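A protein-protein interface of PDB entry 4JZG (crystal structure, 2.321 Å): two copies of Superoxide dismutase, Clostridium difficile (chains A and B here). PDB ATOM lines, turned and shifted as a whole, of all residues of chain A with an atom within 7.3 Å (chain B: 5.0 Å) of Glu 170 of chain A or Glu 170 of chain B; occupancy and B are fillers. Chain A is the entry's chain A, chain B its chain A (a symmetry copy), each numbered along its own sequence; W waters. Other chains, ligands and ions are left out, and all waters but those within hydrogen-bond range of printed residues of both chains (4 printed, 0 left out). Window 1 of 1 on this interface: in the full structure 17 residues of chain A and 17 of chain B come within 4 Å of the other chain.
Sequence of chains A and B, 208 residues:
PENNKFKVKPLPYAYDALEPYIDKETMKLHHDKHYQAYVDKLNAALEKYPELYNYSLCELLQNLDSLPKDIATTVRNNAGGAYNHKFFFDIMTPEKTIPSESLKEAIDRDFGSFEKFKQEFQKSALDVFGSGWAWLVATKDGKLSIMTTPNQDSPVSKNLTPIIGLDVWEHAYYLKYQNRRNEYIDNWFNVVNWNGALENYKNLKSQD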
ATOM      1  N   THR A  26       9.768 -14.604 -13.389  1.00  0.00           N
ATOM      2  CA  THR A  26      10.769 -15.657 -13.459  1.00  0.00           C
ATOM      3  C   THR A  26      11.394 -15.931 -12.096  1.00  0.00           C
ATOM      4  O   THR A  26      11.499 -17.080 -11.689  1.00  0.00           O
ATOM      5  CB  THR A  26      11.835 -15.325 -14.499  1.00  0.00           C
ATOM      6  OG1 THR A  26      11.235 -15.400 -15.800  1.00  0.00           O
ATOM      7  CG2 THR A  26      13.005 -16.312 -14.415  1.00  0.00           C
ATOM      8  N   HIS A  34      10.713 -24.271  -9.229  1.00  0.00           N
ATOM      9  CA  HIS A  34      11.856 -25.085  -9.624  1.00  0.00           C
ATOM     10  C   HIS A  34      12.777 -25.456  -8.450  1.00  0.00           C
ATOM     11  O   HIS A  34      12.941 -26.631  -8.142  1.00  0.00           O
ATOM     12  CB  HIS A  34      12.636 -24.391 -10.748  1.00  0.00           C
ATOM     13  CG  HIS A  34      11.831 -24.194 -11.993  1.00  0.00           C
ATOM     14  ND1 HIS A  34      11.799 -25.121 -13.012  1.00  0.00           N
ATOM     15  CD2 HIS A  34      11.011 -23.187 -12.376  1.00  0.00           C
ATOM     16  CE1 HIS A  34      11.008 -24.686 -13.976  1.00  0.00           C
ATOM     17  NE2 HIS A  34      10.513 -23.517 -13.614  1.00  0.00           N
ATOM     18  N   TYR A  38      13.265 -29.392  -6.504  1.00  0.00           N
ATOM     19  CA  TYR A  38      14.490 -30.153  -6.276  1.00  0.00           C
ATOM     20  C   TYR A  38      14.637 -30.546  -4.795  1.00  0.00           C
ATOM     21  O   TYR A  38      14.954 -31.684  -4.479  1.00  0.00           O
ATOM     22  CB  TYR A  38      15.726 -29.381  -6.761  1.00  0.00           C
ATOM     23  CG  TYR A  38      15.760 -29.152  -8.262  1.00  0.00           C
ATOM     24  CD1 TYR A  38      15.697 -30.221  -9.150  1.00  0.00           C
ATOM     25  CD2 TYR A  38      15.871 -27.877  -8.790  1.00  0.00           C
ATOM     26  CE1 TYR A  38      15.747 -30.022 -10.530  1.00  0.00           C
ATOM     27  CE2 TYR A  38      15.920 -27.669 -10.164  1.00  0.00           C
ATOM     28  CZ  TYR A  38      15.854 -28.753 -11.032  1.00  0.00           C
ATOM     29  OH  TYR A  38      15.900 -28.568 -12.406  1.00  0.00           O
ATOM     30  N   GLY A 130      21.219 -27.872 -24.949  1.00  0.00           N
ATOM     31  CA  GLY A 130      20.281 -28.453 -24.003  1.00  0.00           C
ATOM     32  C   GLY A 130      20.318 -27.694 -22.688  1.00  0.00           C
ATOM     33  O   GLY A 130      20.669 -26.514 -22.667  1.00  0.00           O
ATOM     34  N   SER A 131      19.948 -28.354 -21.596  1.00  0.00           N
ATOM     35  CA  SER A 131      19.927 -27.704 -20.289  1.00  0.00           C
ATOM     36  C   SER A 131      21.292 -27.799 -19.618  1.00  0.00           C
ATOM     37  O   SER A 131      21.978 -28.818 -19.744  1.00  0.00           O
ATOM     38  CB  SER A 131      18.890 -28.359 -19.391  1.00  0.00           C
ATOM     39  OG  SER A 131      17.640 -28.435 -20.048  1.00  0.00           O
ATOM     40  N   GLY A 132      21.680 -26.758 -18.884  1.00  0.00           N
ATOM     41  CA  GLY A 132      22.964 -26.795 -18.217  1.00  0.00           C
ATOM     42  C   GLY A 132      23.401 -25.501 -17.562  1.00  0.00           C
ATOM     43  O   GLY A 132      22.600 -24.591 -17.369  1.00  0.00           O
ATOM     44  N   ASP A 167      22.842 -20.213 -14.690  1.00  0.00           N
ATOM     45  CA  ASP A 167      21.806 -21.147 -15.123  1.00  0.00           C
ATOM     46  C   ASP A 167      21.403 -20.822 -16.572  1.00  0.00           C
ATOM     47  O   ASP A 167      20.918 -19.727 -16.842  1.00  0.00           O
ATOM     48  CB  ASP A 167      20.594 -21.004 -14.182  1.00  0.00           C
ATOM     49  CG  ASP A 167      19.583 -22.124 -14.330  1.00  0.00           C
ATOM     50  OD1 ASP A 167      19.738 -22.941 -15.254  1.00  0.00           O
ATOM     51  OD2 ASP A 167      18.620 -22.202 -13.521  1.00  0.00           O
ATOM     52  N   VAL A 168      21.639 -21.740 -17.513  1.00  0.00           N
ATOM     53  CA  VAL A 168      21.105 -21.568 -18.871  1.00  0.00           C
ATOM     54  C   VAL A 168      20.022 -22.599 -19.238  1.00  0.00           C
ATOM     55  O   VAL A 168      19.743 -22.820 -20.412  1.00  0.00           O
ATOM     56  CB  VAL A 168      22.199 -21.493 -19.979  1.00  0.00           C
ATOM     57  CG1 VAL A 168      23.062 -20.236 -19.812  1.00  0.00           C
ATOM     58  CG2 VAL A 168      23.063 -22.724 -19.976  1.00  0.00           C
ATOM     59  N   TRP A 169      19.409 -23.229 -18.243  1.00  0.00           N
ATOM     60  CA  TRP A 169      18.144 -23.898 -18.510  1.00  0.00           C
ATOM     61  C   TRP A 169      17.197 -22.835 -19.073  1.00  0.00           C
ATOM     62  O   TRP A 169      17.237 -21.671 -18.661  1.00  0.00           O
ATOM     63  CB  TRP A 169      17.536 -24.478 -17.242  1.00  0.00           C
ATOM     64  CG  TRP A 169      18.158 -25.753 -16.742  1.00  0.00           C
ATOM     65  CD1 TRP A 169      19.474 -25.961 -16.409  1.00  0.00           C
ATOM     66  CD2 TRP A 169      17.472 -26.984 -16.453  1.00  0.00           C
ATOM     67  NE1 TRP A 169      19.644 -27.249 -15.947  1.00  0.00           N
ATOM     68  CE2 TRP A 169      18.434 -27.895 -15.963  1.00  0.00           C
ATOM     69  CE3 TRP A 169      16.139 -27.402 -16.563  1.00  0.00           C
ATOM     70  CZ2 TRP A 169      18.107 -29.196 -15.592  1.00  0.00           C
ATOM     71  CZ3 TRP A 169      15.815 -28.695 -16.196  1.00  0.00           C
ATOM     72  CH2 TRP A 169      16.799 -29.577 -15.709  1.00  0.00           C
ATOM     73  N   GLU A 170      16.335 -23.236 -19.997  1.00  0.00           N
ATOM     74  CA  GLU A 170      15.442 -22.290 -20.655  1.00  0.00           C
ATOM     75  C   GLU A 170      14.453 -21.672 -19.674  1.00  0.00           C
ATOM     76  O   GLU A 170      14.029 -20.537 -19.856  1.00  0.00           O
ATOM     77  CB  GLU A 170      14.737 -22.943 -21.865  1.00  0.00           C
ATOM     78  CG  GLU A 170      15.666 -23.071 -23.075  1.00  0.00           C
ATOM     79  CD  GLU A 170      15.094 -23.918 -24.208  1.00  0.00           C
ATOM     80  OE1 GLU A 170      14.336 -24.870 -23.930  1.00  0.00           O
ATOM     81  OE2 GLU A 170      15.422 -23.636 -25.380  1.00  0.00           O
ATOM     82  N   HIS A 171      14.107 -22.389 -18.614  1.00  0.00           N
ATOM     83  CA  HIS A 171      13.219 -21.787 -17.631  1.00  0.00           C
ATOM     84  C   HIS A 171      13.828 -20.546 -16.970  1.00  0.00           C
ATOM     85  O   HIS A 171      13.112 -19.742 -16.404  1.00  0.00           O
ATOM     86  CB  HIS A 171      12.758 -22.795 -16.573  1.00  0.00           C
ATOM     87  CG  HIS A 171      13.846 -23.289 -15.669  1.00  0.00           C
ATOM     88  ND1 HIS A 171      14.140 -24.628 -15.524  1.00  0.00           N
ATOM     89  CD2 HIS A 171      14.680 -22.629 -14.830  1.00  0.00           C
ATOM     90  CE1 HIS A 171      15.120 -24.772 -14.651  1.00  0.00           C
ATOM     91  NE2 HIS A 171      15.465 -23.577 -14.214  1.00  0.00           N
ATOM     92  N   ALA A 172      15.144 -20.385 -17.043  1.00  0.00           N
ATOM     93  CA  ALA A 172      15.776 -19.251 -16.371  1.00  0.00           C
ATOM     94  C   ALA A 172      15.656 -17.954 -17.177  1.00  0.00           C
ATOM     95  O   ALA A 172      15.878 -16.862 -16.640  1.00  0.00           O
ATOM     96  CB  ALA A 172      17.264 -19.555 -16.054  1.00  0.00           C
ATOM     97  N   TYR A 173      15.324 -18.066 -18.463  1.00  0.00           N
ATOM     98  CA  TYR A 173      15.313 -16.877 -19.306  1.00  0.00           C
ATOM     99  C   TYR A 173      14.191 -16.796 -20.335  1.00  0.00           C
ATOM    100  O   TYR A 173      14.071 -15.792 -21.038  1.00  0.00           O
ATOM    101  CB  TYR A 173      16.660 -16.697 -20.002  1.00  0.00           C
ATOM    102  CG  TYR A 173      17.042 -17.793 -20.981  1.00  0.00           C
ATOM    103  CD1 TYR A 173      16.596 -17.769 -22.297  1.00  0.00           C
ATOM    104  CD2 TYR A 173      17.889 -18.837 -20.594  1.00  0.00           C
ATOM    105  CE1 TYR A 173      16.966 -18.775 -23.200  1.00  0.00           C
ATOM    106  CE2 TYR A 173      18.258 -19.844 -21.483  1.00  0.00           C
ATOM    107  CZ  TYR A 173      17.804 -19.808 -22.785  1.00  0.00           C
ATOM    108  OH  TYR A 173      18.187 -20.808 -23.666  1.00  0.00           O
ATOM    109  N   TYR A 174      13.363 -17.827 -20.434  1.00  0.00           N
ATOM    110  CA  TYR A 174      12.428 -17.872 -21.560  1.00  0.00           C
ATOM    111  C   TYR A 174      11.328 -16.806 -21.514  1.00  0.00           C
ATOM    112  O   TYR A 174      11.010 -16.210 -22.543  1.00  0.00           O
ATOM    113  CB  TYR A 174      11.834 -19.272 -21.793  1.00  0.00           C
ATOM    114  CG  TYR A 174      11.638 -19.499 -23.272  1.00  0.00           C
ATOM    115  CD1 TYR A 174      12.721 -19.797 -24.096  1.00  0.00           C
ATOM    116  CD2 TYR A 174      10.391 -19.344 -23.864  1.00  0.00           C
ATOM    117  CE1 TYR A 174      12.565 -19.958 -25.464  1.00  0.00           C
ATOM    118  CE2 TYR A 174      10.220 -19.519 -25.239  1.00  0.00           C
ATOM    119  CZ  TYR A 174      11.309 -19.822 -26.031  1.00  0.00           C
ATOM    120  OH  TYR A 174      11.147 -19.984 -27.394  1.00  0.00           O
ATOM    121  N   LEU A 175      10.759 -16.558 -20.336  1.00  0.00           N
ATOM    122  CA  LEU A 175       9.699 -15.551 -20.212  1.00  0.00           C
ATOM    123  C   LEU A 175      10.114 -14.181 -20.761  1.00  0.00           C
ATOM    124  O   LEU A 175       9.350 -13.539 -21.471  1.00  0.00           O
ATOM    125  CB  LEU A 175       9.206 -15.423 -18.767  1.00  0.00           C
ATOM    126  CG  LEU A 175       8.458 -16.649 -18.243  1.00  0.00           C
ATOM    127  CD1 LEU A 175       7.843 -16.386 -16.886  1.00  0.00           C
ATOM    128  CD2 LEU A 175       7.381 -17.095 -19.228  1.00  0.00           C
ATOM    129  N   GLN A 178      12.912 -15.216 -24.404  1.00  0.00           N
ATOM    130  CA  GLN A 178      12.589 -16.330 -25.298  1.00  0.00           C
ATOM    131  C   GLN A 178      13.877 -17.032 -25.766  1.00  0.00           C
ATOM    132  O   GLN A 178      14.679 -17.448 -24.939  1.00  0.00           O
ATOM    133  CB  GLN A 178      11.698 -15.882 -26.479  1.00  0.00           C
ATOM    134  CG  GLN A 178      10.330 -15.315 -26.053  1.00  0.00           C
ATOM    135  CD  GLN A 178      10.442 -13.898 -25.472  1.00  0.00           C
ATOM    136  OE1 GLN A 178      10.972 -12.999 -26.119  1.00  0.00           O
ATOM    137  NE2 GLN A 178       9.967 -13.709 -24.248  1.00  0.00           N
ATOM    138  N   ASN A 179      14.090 -17.142 -27.075  1.00  0.00           N
ATOM    139  CA  ASN A 179      15.251 -17.869 -27.592  1.00  0.00           C
ATOM    140  C   ASN A 179      16.537 -17.064 -27.534  1.00  0.00           C
ATOM    141  O   ASN A 179      17.606 -17.575 -27.878  1.00  0.00           O
ATOM    142  CB  ASN A 179      15.017 -18.258 -29.049  1.00  0.00           C
ATOM    143  CG  ASN A 179      14.841 -17.040 -29.940  1.00  0.00           C
ATOM    144  OD1 ASN A 179      13.890 -16.278 -29.768  1.00  0.00           O
ATOM    145  ND2 ASN A 179      15.775 -16.830 -30.867  1.00  0.00           N
ATOM    146  N   ARG A 181      19.148 -16.240 -25.853  1.00  0.00           N
ATOM    147  CA  ARG A 181      19.966 -16.537 -24.682  1.00  0.00           C
ATOM    148  C   ARG A 181      21.149 -15.587 -24.575  1.00  0.00           C
ATOM    149  O   ARG A 181      21.578 -15.250 -23.475  1.00  0.00           O
ATOM    150  CB  ARG A 181      20.452 -17.992 -24.680  1.00  0.00           C
ATOM    151  CG  ARG A 181      21.135 -18.391 -23.368  1.00  0.00           C
ATOM    152  CD  ARG A 181      21.982 -19.652 -23.511  1.00  0.00           C
ATOM    153  NE  ARG A 181      21.189 -20.837 -23.823  1.00  0.00           N
ATOM    154  CZ  ARG A 181      21.715 -22.035 -24.062  1.00  0.00           C
ATOM    155  NH1 ARG A 181      23.032 -22.204 -24.007  1.00  0.00           N
ATOM    156  NH2 ARG A 181      20.929 -23.067 -24.343  1.00  0.00           N
ATOM    157  N   HIS B  34      13.739 -21.513 -33.276  1.00  0.00           N
ATOM    158  CA  HIS B  34      14.381 -22.765 -32.894  1.00  0.00           C
ATOM    159  C   HIS B  34      14.607 -23.722 -34.076  1.00  0.00           C
ATOM    160  O   HIS B  34      15.744 -24.053 -34.393  1.00  0.00           O
ATOM    161  CB  HIS B  34      13.588 -23.443 -31.770  1.00  0.00           C
ATOM    162  CG  HIS B  34      13.516 -22.628 -30.518  1.00  0.00           C
ATOM    163  ND1 HIS B  34      14.445 -22.737 -29.507  1.00  0.00           N
ATOM    164  CD2 HIS B  34      12.641 -21.672 -30.124  1.00  0.00           C
ATOM    165  CE1 HIS B  34      14.135 -21.898 -28.535  1.00  0.00           C
ATOM    166  NE2 HIS B  34      13.047 -21.236 -28.886  1.00  0.00           N
ATOM    167  N   VAL B 168       9.698 -32.012 -25.040  1.00  0.00           N
ATOM    168  CA  VAL B 168       9.614 -31.468 -23.678  1.00  0.00           C
ATOM    169  C   VAL B 168      10.792 -30.550 -23.311  1.00  0.00           C
ATOM    170  O   VAL B 168      11.058 -30.313 -22.138  1.00  0.00           O
ATOM    171  CB  VAL B 168       9.387 -32.548 -22.576  1.00  0.00           C
ATOM    172  CG1 VAL B 168       8.017 -33.219 -22.739  1.00  0.00           C
ATOM    173  CG2 VAL B 168      10.479 -33.581 -22.592  1.00  0.00           C
ATOM    174  N   TRP B 169      11.498 -30.027 -24.307  1.00  0.00           N
ATOM    175  CA  TRP B 169      12.346 -28.875 -24.037  1.00  0.00           C
ATOM    176  C   TRP B 169      11.435 -27.787 -23.462  1.00  0.00           C
ATOM    177  O   TRP B 169      10.275 -27.656 -23.866  1.00  0.00           O
ATOM    178  CB  TRP B 169      13.001 -28.349 -25.306  1.00  0.00           C
ATOM    179  CG  TRP B 169      14.169 -29.146 -25.818  1.00  0.00           C
ATOM    180  CD1 TRP B 169      14.182 -30.475 -26.160  1.00  0.00           C
ATOM    181  CD2 TRP B 169      15.484 -28.643 -26.112  1.00  0.00           C
ATOM    182  NE1 TRP B 169      15.429 -30.827 -26.632  1.00  0.00           N
ATOM    183  CE2 TRP B 169      16.243 -29.724 -26.613  1.00  0.00           C
ATOM    184  CE3 TRP B 169      16.092 -27.386 -25.996  1.00  0.00           C
ATOM    185  CZ2 TRP B 169      17.576 -29.587 -26.991  1.00  0.00           C
ATOM    186  CZ3 TRP B 169      17.417 -27.250 -26.371  1.00  0.00           C
ATOM    187  CH2 TRP B 169      18.143 -28.348 -26.869  1.00  0.00           C
ATOM    188  N   GLU B 170      11.962 -26.999 -22.536  1.00  0.00           N
ATOM    189  CA  GLU B 170      11.161 -25.983 -21.865  1.00  0.00           C
ATOM    190  C   GLU B 170      10.686 -24.908 -22.837  1.00  0.00           C
ATOM    191  O   GLU B 170       9.626 -24.325 -22.644  1.00  0.00           O
ATOM    192  CB  GLU B 170      11.915 -25.388 -20.656  1.00  0.00           C
ATOM    193  CG  GLU B 170      11.915 -26.334 -19.452  1.00  0.00           C
ATOM    194  CD  GLU B 170      12.842 -25.899 -18.321  1.00  0.00           C
ATOM    195  OE1 GLU B 170      13.892 -25.285 -18.601  1.00  0.00           O
ATOM    196  OE2 GLU B 170      12.522 -26.191 -17.149  1.00  0.00           O
ATOM    197  N   HIS B 171      11.440 -24.662 -23.899  1.00  0.00           N
ATOM    198  CA  HIS B 171      10.966 -23.690 -24.873  1.00  0.00           C
ATOM    199  C   HIS B 171       9.648 -24.108 -25.529  1.00  0.00           C
ATOM    200  O   HIS B 171       8.951 -23.279 -26.086  1.00  0.00           O
ATOM    201  CB  HIS B 171      12.025 -23.372 -25.935  1.00  0.00           C
ATOM    202  CG  HIS B 171      12.351 -24.514 -26.849  1.00  0.00           C
ATOM    203  ND1 HIS B 171      13.632 -24.999 -27.005  1.00  0.00           N
ATOM    204  CD2 HIS B 171      11.572 -25.238 -27.688  1.00  0.00           C
ATOM    205  CE1 HIS B 171      13.627 -25.983 -27.884  1.00  0.00           C
ATOM    206  NE2 HIS B 171      12.392 -26.148 -28.315  1.00  0.00           N
ATOM    207  N   ALA B 172       9.297 -25.387 -25.463  1.00  0.00           N
ATOM    208  CA  ALA B 172       8.080 -25.844 -26.131  1.00  0.00           C
ATOM    209  C   ALA B 172       6.819 -25.541 -25.315  1.00  0.00           C
ATOM    210  O   ALA B 172       5.702 -25.599 -25.845  1.00  0.00           O
ATOM    211  CB  ALA B 172       8.163 -27.357 -26.458  1.00  0.00           C
ATOM    212  N   TYR B 173       6.985 -25.239 -24.028  1.00  0.00           N
ATOM    213  CA  TYR B 173       5.815 -25.060 -23.177  1.00  0.00           C
ATOM    214  C   TYR B 173       5.903 -23.945 -22.141  1.00  0.00           C
ATOM    215  O   TYR B 173       4.932 -23.686 -21.430  1.00  0.00           O
ATOM    216  CB  TYR B 173       5.446 -26.372 -22.488  1.00  0.00           C
ATOM    217  CG  TYR B 173       6.480 -26.915 -21.518  1.00  0.00           C
ATOM    218  CD1 TYR B 173       6.529 -26.480 -20.199  1.00  0.00           C
ATOM    219  CD2 TYR B 173       7.388 -27.903 -21.917  1.00  0.00           C
ATOM    220  CE1 TYR B 173       7.476 -26.998 -19.305  1.00  0.00           C
ATOM    221  CE2 TYR B 173       8.336 -28.419 -21.038  1.00  0.00           C
ATOM    222  CZ  TYR B 173       8.374 -27.974 -19.733  1.00  0.00           C
ATOM    223  OH  TYR B 173       9.313 -28.503 -18.861  1.00  0.00           O
ATOM    224  N   TYR B 174       7.045 -23.277 -22.044  1.00  0.00           N
ATOM    225  CA  TYR B 174       7.231 -22.366 -20.913  1.00  0.00           C
ATOM    226  C   TYR B 174       6.336 -21.122 -20.945  1.00  0.00           C
ATOM    227  O   TYR B 174       5.799 -20.728 -19.910  1.00  0.00           O
ATOM    228  CB  TYR B 174       8.704 -21.983 -20.686  1.00  0.00           C
ATOM    229  CG  TYR B 174       8.966 -21.831 -19.207  1.00  0.00           C
ATOM    230  CD1 TYR B 174       9.109 -22.952 -18.392  1.00  0.00           C
ATOM    231  CD2 TYR B 174       8.997 -20.580 -18.607  1.00  0.00           C
ATOM    232  CE1 TYR B 174       9.298 -22.831 -17.024  1.00  0.00           C
ATOM    233  CE2 TYR B 174       9.203 -20.445 -17.232  1.00  0.00           C
ATOM    234  CZ  TYR B 174       9.350 -21.572 -16.449  1.00  0.00           C
ATOM    235  OH  TYR B 174       9.542 -21.444 -15.086  1.00  0.00           O
HETATM  236  O   HOH W   1      16.036 -26.159 -20.147  1.00  0.00           O
HETATM  237  O   HOH W   2       9.186 -21.686 -28.396  1.00  0.00           O
HETATM  238  O   HOH W   3      14.899 -27.129 -22.404  1.00  0.00           O
HETATM  239  O   HOH W   4      11.516 -19.758 -14.084  1.00  0.00           O
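Among the printed residues, merely in contact across the chains: His 34 of chain A with Glu 170 of chain B (3.8 Å), Gly 130 of chain A with Trp 169 of chain B (3.6 Å), Trp 169 of chain A with Glu 170 of chain B (3.7 Å), Glu 170 of chain A with His 34 of chain B (3.8 Å), Glu 170 of chain A with Trp 169 of chain B (3.7 Å), His 171 of chain A with Tyr 174 of chain B (3.5 Å), Tyr 174 of chain A with His 171 of chain B (3.5 Å), Leu 175 of chain A with Tyr 174 of chain B (3.9 Å) and Asn 179 of chain A with His 34 of chain B (3.6 Å).
A ring nitrogen (ND1) of His 34 of chain A sits at hydrogen-bond distance from a ring nitrogen (ND1) of His 171 of chain A, 3.5 Å away. N of Trp 169 of chain A sits at hydrogen-bond distance from OD1 of Asp 167 of chain A (3.0 Å). The backbone carbonyl oxygen of Tyr 174 of chain A lies close to the side-chain amide nitrogen of Gln 178 of chain A. The backbone carbonyl oxygen (O) of Leu 175 of chain A sits at hydrogen-bond distance from the side-chain amide nitrogen (NE2) of Gln 178 of chain A (2.8 Å). A ring nitrogen (ND1) of His 171 of chain B sits at hydrogen-bond distance from a ring nitrogen (ND1) of His 34 of chain B (3.5 Å).
Printed residues of chain B within 4 Å of His 34 of chain A: Glu 170 and Tyr 174. Of chain B, only His 34 (3.8 Å), Trp 169 (3.7 Å), Glu 170 (3.5 Å) and His 171 (2.8 Å) come within 4 Å of Glu 170 of chain A. Of the printed residues of chain B, His 171 of chain A touches Glu 170 (2.8 Å) and Tyr 174 (3.5 Å). Of the printed residues of chain B, Tyr 174 of chain A touches His 34 (2.7 Å) and His 171 (3.5 Å). Of the printed residues of chain B, Leu 175 of chain A touches Tyr 174 (3.9 Å). Of the printed residues of chain B, Asn 179 of chain A touches His 34 (3.6 Å). Glu 170 of chain B touches four residues of chain A. Ala 172 of chain B touches none of the printed residues of chain A. The nearest printed residue of chain B that does not touch Glu 170 of chain A is Tyr 174 of chain B (5.2 Å). The nearest residue of chain A that does not touch Glu 170 of chain B is Ser 131 of chain A (5.1 Å).
Water W2 lies within hydrogen-bond range of the side-chain hydroxyl of Tyr 174 of chain A and the backbone carbonyl oxygen of His 171 of chain B. Water W4 lies within hydrogen-bond range of the side-chain hydroxyl (OH) of Tyr 174 of chain B (2.8 Å) and the backbone carbonyl oxygen (O) of His 171 of chain A (2.8 Å). Water W1 lies within hydrogen-bond range of the side-chain carboxylate of Glu 170 of chain B (2.8 Å), the side-chain hydroxyl of Ser 131 of chain A (2.8 Å) and the backbone NH of Glu 170 of chain A (2.9 Å). Water W3 lies within hydrogen-bond range of OE1 of Glu 170 of chain A (2.8 Å) and N of Glu 170 of chain B (2.9 Å).
A ring nitrogen (NE2) of His 34 of chain A lies within hydrogen-bond range of the side-chain hydroxyl (OH) of Tyr 174 of chain B (2.7 Å). The side-chain carboxylate (OE1) of Glu 170 of chain A lies within hydrogen-bond range of the backbone NH (N) of Glu 170 of chain B, 3.5 Å away. OE2 of Glu 170 of chain A lies within hydrogen-bond range of ND1 of His 171 of chain B (2.8 Å). ND1 of His 171 of chain A sits at hydrogen-bond distance from OE2 of Glu 170 of chain B. A ring nitrogen (NE2) of His 34 of chain B sits at hydrogen-bond distance from the side-chain hydroxyl (OH) of Tyr 174 of chain A (2.7 Å).
Of the 18 printed residues of chain A, 8 touch a printed residue of chain B. Printed residues of chain A that touch a printed residue of chain B: His 34, Gly 130, Trp 169, Glu 170, His 171, Tyr 174, Leu 175 and Asn 179. Hydrophobic or aromatic side chains of chain A within 4 Å of the printed part of chain B: His 34, Trp 169, His 171, Tyr 174 and Leu 175. Printed residues of chain B that touch a printed residue of chain A: His 34, Trp 169, Glu 170, His 171 and Tyr 174. Hydrophobic or aromatic side chains of chain B that line the printed part of chain A: His 34, Trp 169, His 171 and Tyr 174. Among the printed residues, 14 pairs touch across the chains.
His 34 of chain A touches Glu 170 of chain B, and with the chains exchanged Glu 170 of chain A touches His 34 of chain B. Glu 170 of chain B touches its own counterpart, Glu 170 of chain A. Glu 170 of chain A touches His 171 of chain B, and with the chains exchanged His 171 of chain A touches Glu 170 of chain B. His 171 of chain A touches Tyr 174 of chain B, and with the chains exchanged Tyr 174 of chain A touches His 171 of chain B. Positions printed for both chains: 34, 168, 169, 170, 171, 172, 173 and 174. Of the 14 pairs that touch across the chains among the printed residues, 11 have their exchanged pair printed and touching as well.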
